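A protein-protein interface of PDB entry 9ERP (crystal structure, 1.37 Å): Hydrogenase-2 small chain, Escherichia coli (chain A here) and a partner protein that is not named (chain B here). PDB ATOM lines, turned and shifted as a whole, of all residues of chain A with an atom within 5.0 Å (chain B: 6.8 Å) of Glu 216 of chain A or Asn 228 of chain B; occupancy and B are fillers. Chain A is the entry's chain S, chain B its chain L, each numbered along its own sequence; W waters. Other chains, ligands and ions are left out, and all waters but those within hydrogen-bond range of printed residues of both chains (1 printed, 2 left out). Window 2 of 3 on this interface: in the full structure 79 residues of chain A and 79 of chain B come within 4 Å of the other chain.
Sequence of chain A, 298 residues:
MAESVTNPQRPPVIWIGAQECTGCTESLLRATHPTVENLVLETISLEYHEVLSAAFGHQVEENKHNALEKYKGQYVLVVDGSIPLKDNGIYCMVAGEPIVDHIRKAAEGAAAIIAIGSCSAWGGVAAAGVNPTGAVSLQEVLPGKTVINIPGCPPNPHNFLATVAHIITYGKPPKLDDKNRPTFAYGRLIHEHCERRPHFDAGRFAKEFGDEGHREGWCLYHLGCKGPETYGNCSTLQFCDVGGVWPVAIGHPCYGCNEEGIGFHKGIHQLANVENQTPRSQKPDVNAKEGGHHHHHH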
ATOM      1  N   GLU A 212     -30.793  17.236  24.501  1.00  0.00           N
ATOM      2  CA  GLU A 212     -30.970  16.418  23.302  1.00  0.00           C
ATOM      3  C   GLU A 212     -30.674  17.218  22.036  1.00  0.00           C
ATOM      4  O   GLU A 212     -29.968  16.743  21.146  1.00  0.00           O
ATOM      5  CB  GLU A 212     -32.388  15.846  23.238  1.00  0.00           C
ATOM      6  CG  GLU A 212     -32.538  14.553  23.994  1.00  0.00           C
ATOM      7  CD  GLU A 212     -33.903  13.917  23.801  1.00  0.00           C
ATOM      8  OE1 GLU A 212     -34.797  14.547  23.187  1.00  0.00           O
ATOM      9  OE2 GLU A 212     -34.061  12.780  24.282  1.00  0.00           O
ATOM     10  N   GLY A 213     -31.205  18.438  21.947  1.00  0.00           N
ATOM     11  CA  GLY A 213     -30.990  19.236  20.755  1.00  0.00           C
ATOM     12  C   GLY A 213     -29.532  19.616  20.574  1.00  0.00           C
ATOM     13  O   GLY A 213     -29.009  19.596  19.453  1.00  0.00           O
ATOM     14  N   HIS A 214     -28.872  19.991  21.667  1.00  0.00           N
ATOM     15  CA  HIS A 214     -27.439  20.256  21.618  1.00  0.00           C
ATOM     16  C   HIS A 214     -26.687  19.060  21.066  1.00  0.00           C
ATOM     17  O   HIS A 214     -25.750  19.217  20.262  1.00  0.00           O
ATOM     18  CB  HIS A 214     -26.970  20.566  23.038  1.00  0.00           C
ATOM     19  CG  HIS A 214     -25.560  21.056  23.119  1.00  0.00           C
ATOM     20  ND1 HIS A 214     -24.618  20.425  23.903  1.00  0.00           N
ATOM     21  CD2 HIS A 214     -24.940  22.119  22.560  1.00  0.00           C
ATOM     22  CE1 HIS A 214     -23.469  21.070  23.808  1.00  0.00           C
ATOM     23  NE2 HIS A 214     -23.638  22.103  22.994  1.00  0.00           N
ATOM     24  N   ARG A 215     -27.061  17.859  21.483  1.00  0.00           N
ATOM     25  CA  ARG A 215     -26.389  16.645  21.048  1.00  0.00           C
ATOM     26  C   ARG A 215     -26.821  16.207  19.654  1.00  0.00           C
ATOM     27  O   ARG A 215     -26.276  15.236  19.130  1.00  0.00           O
ATOM     28  CB  ARG A 215     -26.593  15.552  22.093  1.00  0.00           C
ATOM     29  CG  ARG A 215     -25.835  15.872  23.399  1.00  0.00           C
ATOM     30  CD  ARG A 215     -26.114  14.846  24.503  1.00  0.00           C
ATOM     31  NE  ARG A 215     -25.568  13.557  24.118  1.00  0.00           N
ATOM     32  CZ  ARG A 215     -26.285  12.464  23.875  1.00  0.00           C
ATOM     33  NH1 ARG A 215     -27.591  12.423  24.134  1.00  0.00           N
ATOM     34  NH2 ARG A 215     -25.679  11.391  23.356  1.00  0.00           N
ATOM     35  N   GLU A 216     -27.743  16.932  19.034  1.00  0.00           N
ATOM     36  CA  GLU A 216     -28.050  16.746  17.627  1.00  0.00           C
ATOM     37  C   GLU A 216     -27.492  17.868  16.753  1.00  0.00           C
ATOM     38  O   GLU A 216     -27.759  17.885  15.550  1.00  0.00           O
ATOM     39  CB  GLU A 216     -29.557  16.597  17.446  1.00  0.00           C
ATOM     40  CG  GLU A 216     -30.154  15.323  18.077  1.00  0.00           C
ATOM     41  CD  GLU A 216     -29.498  14.011  17.618  1.00  0.00           C
ATOM     42  OE1 GLU A 216     -28.972  13.930  16.474  1.00  0.00           O
ATOM     43  OE2 GLU A 216     -29.515  13.040  18.411  1.00  0.00           O
ATOM     44  N   GLY A 217     -26.712  18.788  17.319  1.00  0.00           N
ATOM     45  CA  GLY A 217     -26.145  19.854  16.541  1.00  0.00           C
ATOM     46  C   GLY A 217     -27.109  20.940  16.163  1.00  0.00           C
ATOM     47  O   GLY A 217     -26.927  21.574  15.124  1.00  0.00           O
ATOM     48  N   TRP A 218     -28.117  21.205  16.988  1.00  0.00           N
ATOM     49  CA  TRP A 218     -29.090  22.232  16.663  1.00  0.00           C
ATOM     50  C   TRP A 218     -28.545  23.640  16.907  1.00  0.00           C
ATOM     51  O   TRP A 218     -27.420  23.850  17.387  1.00  0.00           O
ATOM     52  CB  TRP A 218     -30.349  22.013  17.492  1.00  0.00           C
ATOM     53  CG  TRP A 218     -31.176  20.857  17.038  1.00  0.00           C
ATOM     54  CD1 TRP A 218     -30.914  20.009  16.002  1.00  0.00           C
ATOM     55  CD2 TRP A 218     -32.402  20.414  17.622  1.00  0.00           C
ATOM     56  NE1 TRP A 218     -31.910  19.064  15.906  1.00  0.00           N
ATOM     57  CE2 TRP A 218     -32.827  19.299  16.900  1.00  0.00           C
ATOM     58  CE3 TRP A 218     -33.173  20.861  18.694  1.00  0.00           C
ATOM     59  CZ2 TRP A 218     -34.022  18.617  17.201  1.00  0.00           C
ATOM     60  CZ3 TRP A 218     -34.359  20.189  18.994  1.00  0.00           C
ATOM     61  CH2 TRP A 218     -34.750  19.073  18.260  1.00  0.00           C
ATOM     62  N   PRO B 226     -20.801  18.326  22.698  1.00  0.00           N
ATOM     63  CA  PRO B 226     -21.929  17.393  22.817  1.00  0.00           C
ATOM     64  C   PRO B 226     -21.472  16.000  22.442  1.00  0.00           C
ATOM     65  O   PRO B 226     -21.152  15.766  21.270  1.00  0.00           O
ATOM     66  CB  PRO B 226     -22.935  17.915  21.776  1.00  0.00           C
ATOM     67  CG  PRO B 226     -22.237  19.084  21.059  1.00  0.00           C
ATOM     68  CD  PRO B 226     -20.768  18.944  21.359  1.00  0.00           C
ATOM     69  N   ILE B 227     -21.362  15.093  23.404  1.00  0.00           N
ATOM     70  CA  ILE B 227     -20.887  13.741  23.117  1.00  0.00           C
ATOM     71  C   ILE B 227     -22.040  12.920  22.555  1.00  0.00           C
ATOM     72  O   ILE B 227     -23.058  12.732  23.223  1.00  0.00           O
ATOM     73  CB  ILE B 227     -20.301  13.071  24.364  1.00  0.00           C
ATOM     74  CG1 ILE B 227     -18.988  13.747  24.777  1.00  0.00           C
ATOM     75  CG2 ILE B 227     -20.099  11.571  24.114  1.00  0.00           C
ATOM     76  CD1 ILE B 227     -18.464  13.282  26.139  1.00  0.00           C
ATOM     77  N   ASN B 228     -21.864  12.405  21.342  1.00  0.00           N
ATOM     78  CA  ASN B 228     -22.873  11.535  20.737  1.00  0.00           C
ATOM     79  C   ASN B 228     -22.170  10.767  19.619  1.00  0.00           C
ATOM     80  O   ASN B 228     -22.020  11.294  18.518  1.00  0.00           O
ATOM     81  CB  ASN B 228     -24.034  12.342  20.191  1.00  0.00           C
ATOM     82  CG  ASN B 228     -25.143  11.473  19.663  1.00  0.00           C
ATOM     83  OD1 ASN B 228     -25.019  10.253  19.605  1.00  0.00           O
ATOM     84  ND2 ASN B 228     -26.232  12.110  19.261  1.00  0.00           N
ATOM     85  N   LEU B 229     -21.750   9.534  19.915  1.00  0.00           N
ATOM     86  CA  LEU B 229     -21.034   8.728  18.921  1.00  0.00           C
ATOM     87  C   LEU B 229     -21.784   8.652  17.601  1.00  0.00           C
ATOM     88  O   LEU B 229     -21.156   8.505  16.542  1.00  0.00           O
ATOM     89  CB  LEU B 229     -20.799   7.321  19.461  1.00  0.00           C
ATOM     90  CG  LEU B 229     -19.862   7.200  20.649  1.00  0.00           C
ATOM     91  CD1 LEU B 229     -19.643   5.730  20.971  1.00  0.00           C
ATOM     92  CD2 LEU B 229     -18.516   7.870  20.414  1.00  0.00           C
ATOM     93  N   ASP B 230     -23.113   8.786  17.625  1.00  0.00           N
ATOM     94  CA  ASP B 230     -23.948   8.568  16.448  1.00  0.00           C
ATOM     95  C   ASP B 230     -24.548   9.845  15.901  1.00  0.00           C
ATOM     96  O   ASP B 230     -25.395   9.790  14.994  1.00  0.00           O
ATOM     97  CB  ASP B 230     -25.036   7.539  16.777  1.00  0.00           C
ATOM     98  CG  ASP B 230     -24.452   6.210  17.099  1.00  0.00           C
ATOM     99  OD1 ASP B 230     -23.911   5.557  16.189  1.00  0.00           O
ATOM    100  OD2 ASP B 230     -24.507   5.813  18.292  1.00  0.00           O
ATOM    101  N   GLY B 231     -24.116  10.995  16.423  1.00  0.00           N
ATOM    102  CA  GLY B 231     -24.683  12.264  16.031  1.00  0.00           C
ATOM    103  C   GLY B 231     -23.914  12.937  14.902  1.00  0.00           C
ATOM    104  O   GLY B 231     -22.693  12.972  14.892  1.00  0.00           O
ATOM    105  N   LEU B 232     -24.660  13.490  13.963  1.00  0.00           N
ATOM    106  CA  LEU B 232     -24.098  14.353  12.941  1.00  0.00           C
ATOM    107  C   LEU B 232     -23.817  15.741  13.524  1.00  0.00           C
ATOM    108  O   LEU B 232     -24.632  16.313  14.248  1.00  0.00           O
ATOM    109  CB  LEU B 232     -25.106  14.439  11.786  1.00  0.00           C
ATOM    110  CG  LEU B 232     -24.621  15.114  10.507  1.00  0.00           C
ATOM    111  CD1 LEU B 232     -25.246  14.412   9.303  1.00  0.00           C
ATOM    112  CD2 LEU B 232     -24.961  16.595  10.529  1.00  0.00           C
ATOM    113  N   GLY B 233     -22.627  16.285  13.210  1.00  0.00           N
ATOM    114  CA  GLY B 233     -22.260  17.627  13.599  1.00  0.00           C
ATOM    115  C   GLY B 233     -21.848  17.822  15.047  1.00  0.00           C
ATOM    116  O   GLY B 233     -21.740  18.972  15.484  1.00  0.00           O
ATOM    117  N   VAL B 234     -21.619  16.752  15.802  1.00  0.00           N
ATOM    118  CA  VAL B 234     -21.259  16.826  17.214  1.00  0.00           C
ATOM    119  C   VAL B 234     -20.025  15.966  17.461  1.00  0.00           C
ATOM    120  O   VAL B 234     -19.391  15.481  16.513  1.00  0.00           O
ATOM    121  CB  VAL B 234     -22.442  16.452  18.126  1.00  0.00           C
ATOM    122  CG1 VAL B 234     -23.610  17.387  17.871  1.00  0.00           C
ATOM    123  CG2 VAL B 234     -22.871  15.037  17.939  1.00  0.00           C
ATOM    124  N   LEU B 235     -19.658  15.773  18.728  1.00  0.00           N
ATOM    125  CA  LEU B 235     -18.448  15.012  19.067  1.00  0.00           C
ATOM    126  C   LEU B 235     -18.800  13.534  18.963  1.00  0.00           C
ATOM    127  O   LEU B 235     -19.286  12.917  19.911  1.00  0.00           O
ATOM    128  CB  LEU B 235     -17.934  15.396  20.444  1.00  0.00           C
ATOM    129  CG  LEU B 235     -16.614  14.756  20.885  1.00  0.00           C
ATOM    130  CD1 LEU B 235     -15.528  15.056  19.888  1.00  0.00           C
ATOM    131  CD2 LEU B 235     -16.195  15.212  22.253  1.00  0.00           C
ATOM    132  N   ASN B 236     -18.557  12.957  17.783  1.00  0.00           N
ATOM    133  CA  ASN B 236     -18.869  11.567  17.451  1.00  0.00           C
ATOM    134  C   ASN B 236     -17.575  10.769  17.328  1.00  0.00           C
ATOM    135  O   ASN B 236     -16.484  11.250  17.639  1.00  0.00           O
ATOM    136  CB  ASN B 236     -19.762  11.535  16.209  1.00  0.00           C
ATOM    137  CG  ASN B 236     -19.096  12.145  15.004  1.00  0.00           C
ATOM    138  OD1 ASN B 236     -17.878  12.085  14.870  1.00  0.00           O
ATOM    139  ND2 ASN B 236     -19.891  12.698  14.108  1.00  0.00           N
ATOM    140  N   LEU B 237     -17.688   9.506  16.916  1.00  0.00           N
ATOM    141  CA  LEU B 237     -16.488   8.672  16.873  1.00  0.00           C
ATOM    142  C   LEU B 237     -15.509   9.167  15.810  1.00  0.00           C
ATOM    143  O   LEU B 237     -14.287   9.118  16.008  1.00  0.00           O
ATOM    144  CB  LEU B 237     -16.874   7.203  16.670  1.00  0.00           C
ATOM    145  CG  LEU B 237     -15.720   6.223  16.771  1.00  0.00           C
ATOM    146  CD1 LEU B 237     -15.030   6.346  18.143  1.00  0.00           C
ATOM    147  CD2 LEU B 237     -16.217   4.814  16.536  1.00  0.00           C
ATOM    148  N   ILE B 450     -17.433   6.717  27.400  1.00  0.00           N
ATOM    149  CA  ILE B 450     -18.528   6.867  26.454  1.00  0.00           C
ATOM    150  C   ILE B 450     -19.104   5.500  26.119  1.00  0.00           C
ATOM    151  O   ILE B 450     -20.323   5.334  26.010  1.00  0.00           O
ATOM    152  CB  ILE B 450     -18.072   7.618  25.190  1.00  0.00           C
ATOM    153  CG1 ILE B 450     -17.638   9.046  25.529  1.00  0.00           C
ATOM    154  CG2 ILE B 450     -19.195   7.634  24.130  1.00  0.00           C
ATOM    155  CD1 ILE B 450     -16.953   9.768  24.344  1.00  0.00           C
ATOM    156  N   HIS B 455     -22.626   9.840  28.402  1.00  0.00           N
ATOM    157  CA  HIS B 455     -22.417  10.949  27.479  1.00  0.00           C
ATOM    158  C   HIS B 455     -22.605  12.295  28.153  1.00  0.00           C
ATOM    159  O   HIS B 455     -22.725  13.310  27.463  1.00  0.00           O
ATOM    160  CB  HIS B 455     -23.365  10.817  26.283  1.00  0.00           C
ATOM    161  CG  HIS B 455     -24.816  10.884  26.655  1.00  0.00           C
ATOM    162  ND1 HIS B 455     -25.649   9.784  26.607  1.00  0.00           N
ATOM    163  CD2 HIS B 455     -25.580  11.918  27.078  1.00  0.00           C
ATOM    164  CE1 HIS B 455     -26.861  10.137  26.992  1.00  0.00           C
ATOM    165  NE2 HIS B 455     -26.850  11.426  27.286  1.00  0.00           N
HETATM  166  O   HOH W   1     -27.244  14.875  14.594  1.00  0.00           O
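Glu 216 of chain A touches just these residues of chain B: Asn 228 and Leu 232.
Of chain A, only Arg 215 (3.1 Å) and Glu 216 (3.5 Å) come within 4 Å of Asn 228 of chain B.
Of the printed residues of chain A, Val 234 of chain B touches His 214, Arg 215 and Gly 217.
Printed residues of chain B within 4 Å of His 214 of chain A: Pro 226 and Val 234.
Leu 237 of chain B touches none of the printed residues of chain A.
Water W1 lies within hydrogen-bond range of the side-chain carboxylate of Glu 216 of chain A (2.7 Å) and the backbone NH of Leu 232 of chain B (3.0 Å).
Among the printed residues, merely in contact across the chains: Gly 217 of chain A with Val 234 of chain B (3.4 Å), His 214 of chain A with Pro 226 of chain B (3.5 Å), Glu 216 of chain A with Asn 228 of chain B (3.5 Å), Arg 215 of chain A with Val 234 of chain B (3.6 Å), His 214 of chain A with Val 234 of chain B (3.7 Å), Glu 216 of chain A with Leu 232 of chain B (3.7 Å) and Arg 215 of chain A with Pro 226 of chain B (3.8 Å).
The backbone carbonyl oxygen (O) of Ile 227 of chain B lies within hydrogen-bond range of the guanidinium group (NE) of Arg 215 of chain A, 2.8 Å away.
The backbone carbonyl oxygen (O) of Arg 215 of chain A sits at hydrogen-bond distance from the side-chain amide nitrogen (ND2) of Asn 228 of chain B, at 3.1 Å.
NH1 of Arg 215 of chain A is in hydrogen-bond range of NE2 of His 455 of chain B, 3.4 Å away.
The side-chain amide oxygen of Asn 228 of chain B lies within hydrogen-bond range of the backbone NH of Gly 231 of chain B (3.4 Å).
The backbone NH (N) of Leu 235 of chain B lies within hydrogen-bond range of the backbone carbonyl oxygen (O) of Pro 226 of chain B (2.9 Å).
The backbone NH (N) of Asp 230 of chain B lies close to the side-chain amide oxygen (OD1) of Asn 228 of chain B (3.1 Å).
The backbone NH (N) of Asn 228 of chain B lies within hydrogen-bond range of the backbone carbonyl oxygen (O) of Leu 235 of chain B (3.0 Å).
Hydrophobic or aromatic side chains of chain A within 4 Å of the printed part of chain B: His 214.
Among the printed residues, no Asp or Glu carboxylate lies within 4 Å of a Lys or Arg side-chain nitrogen of the other chain.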
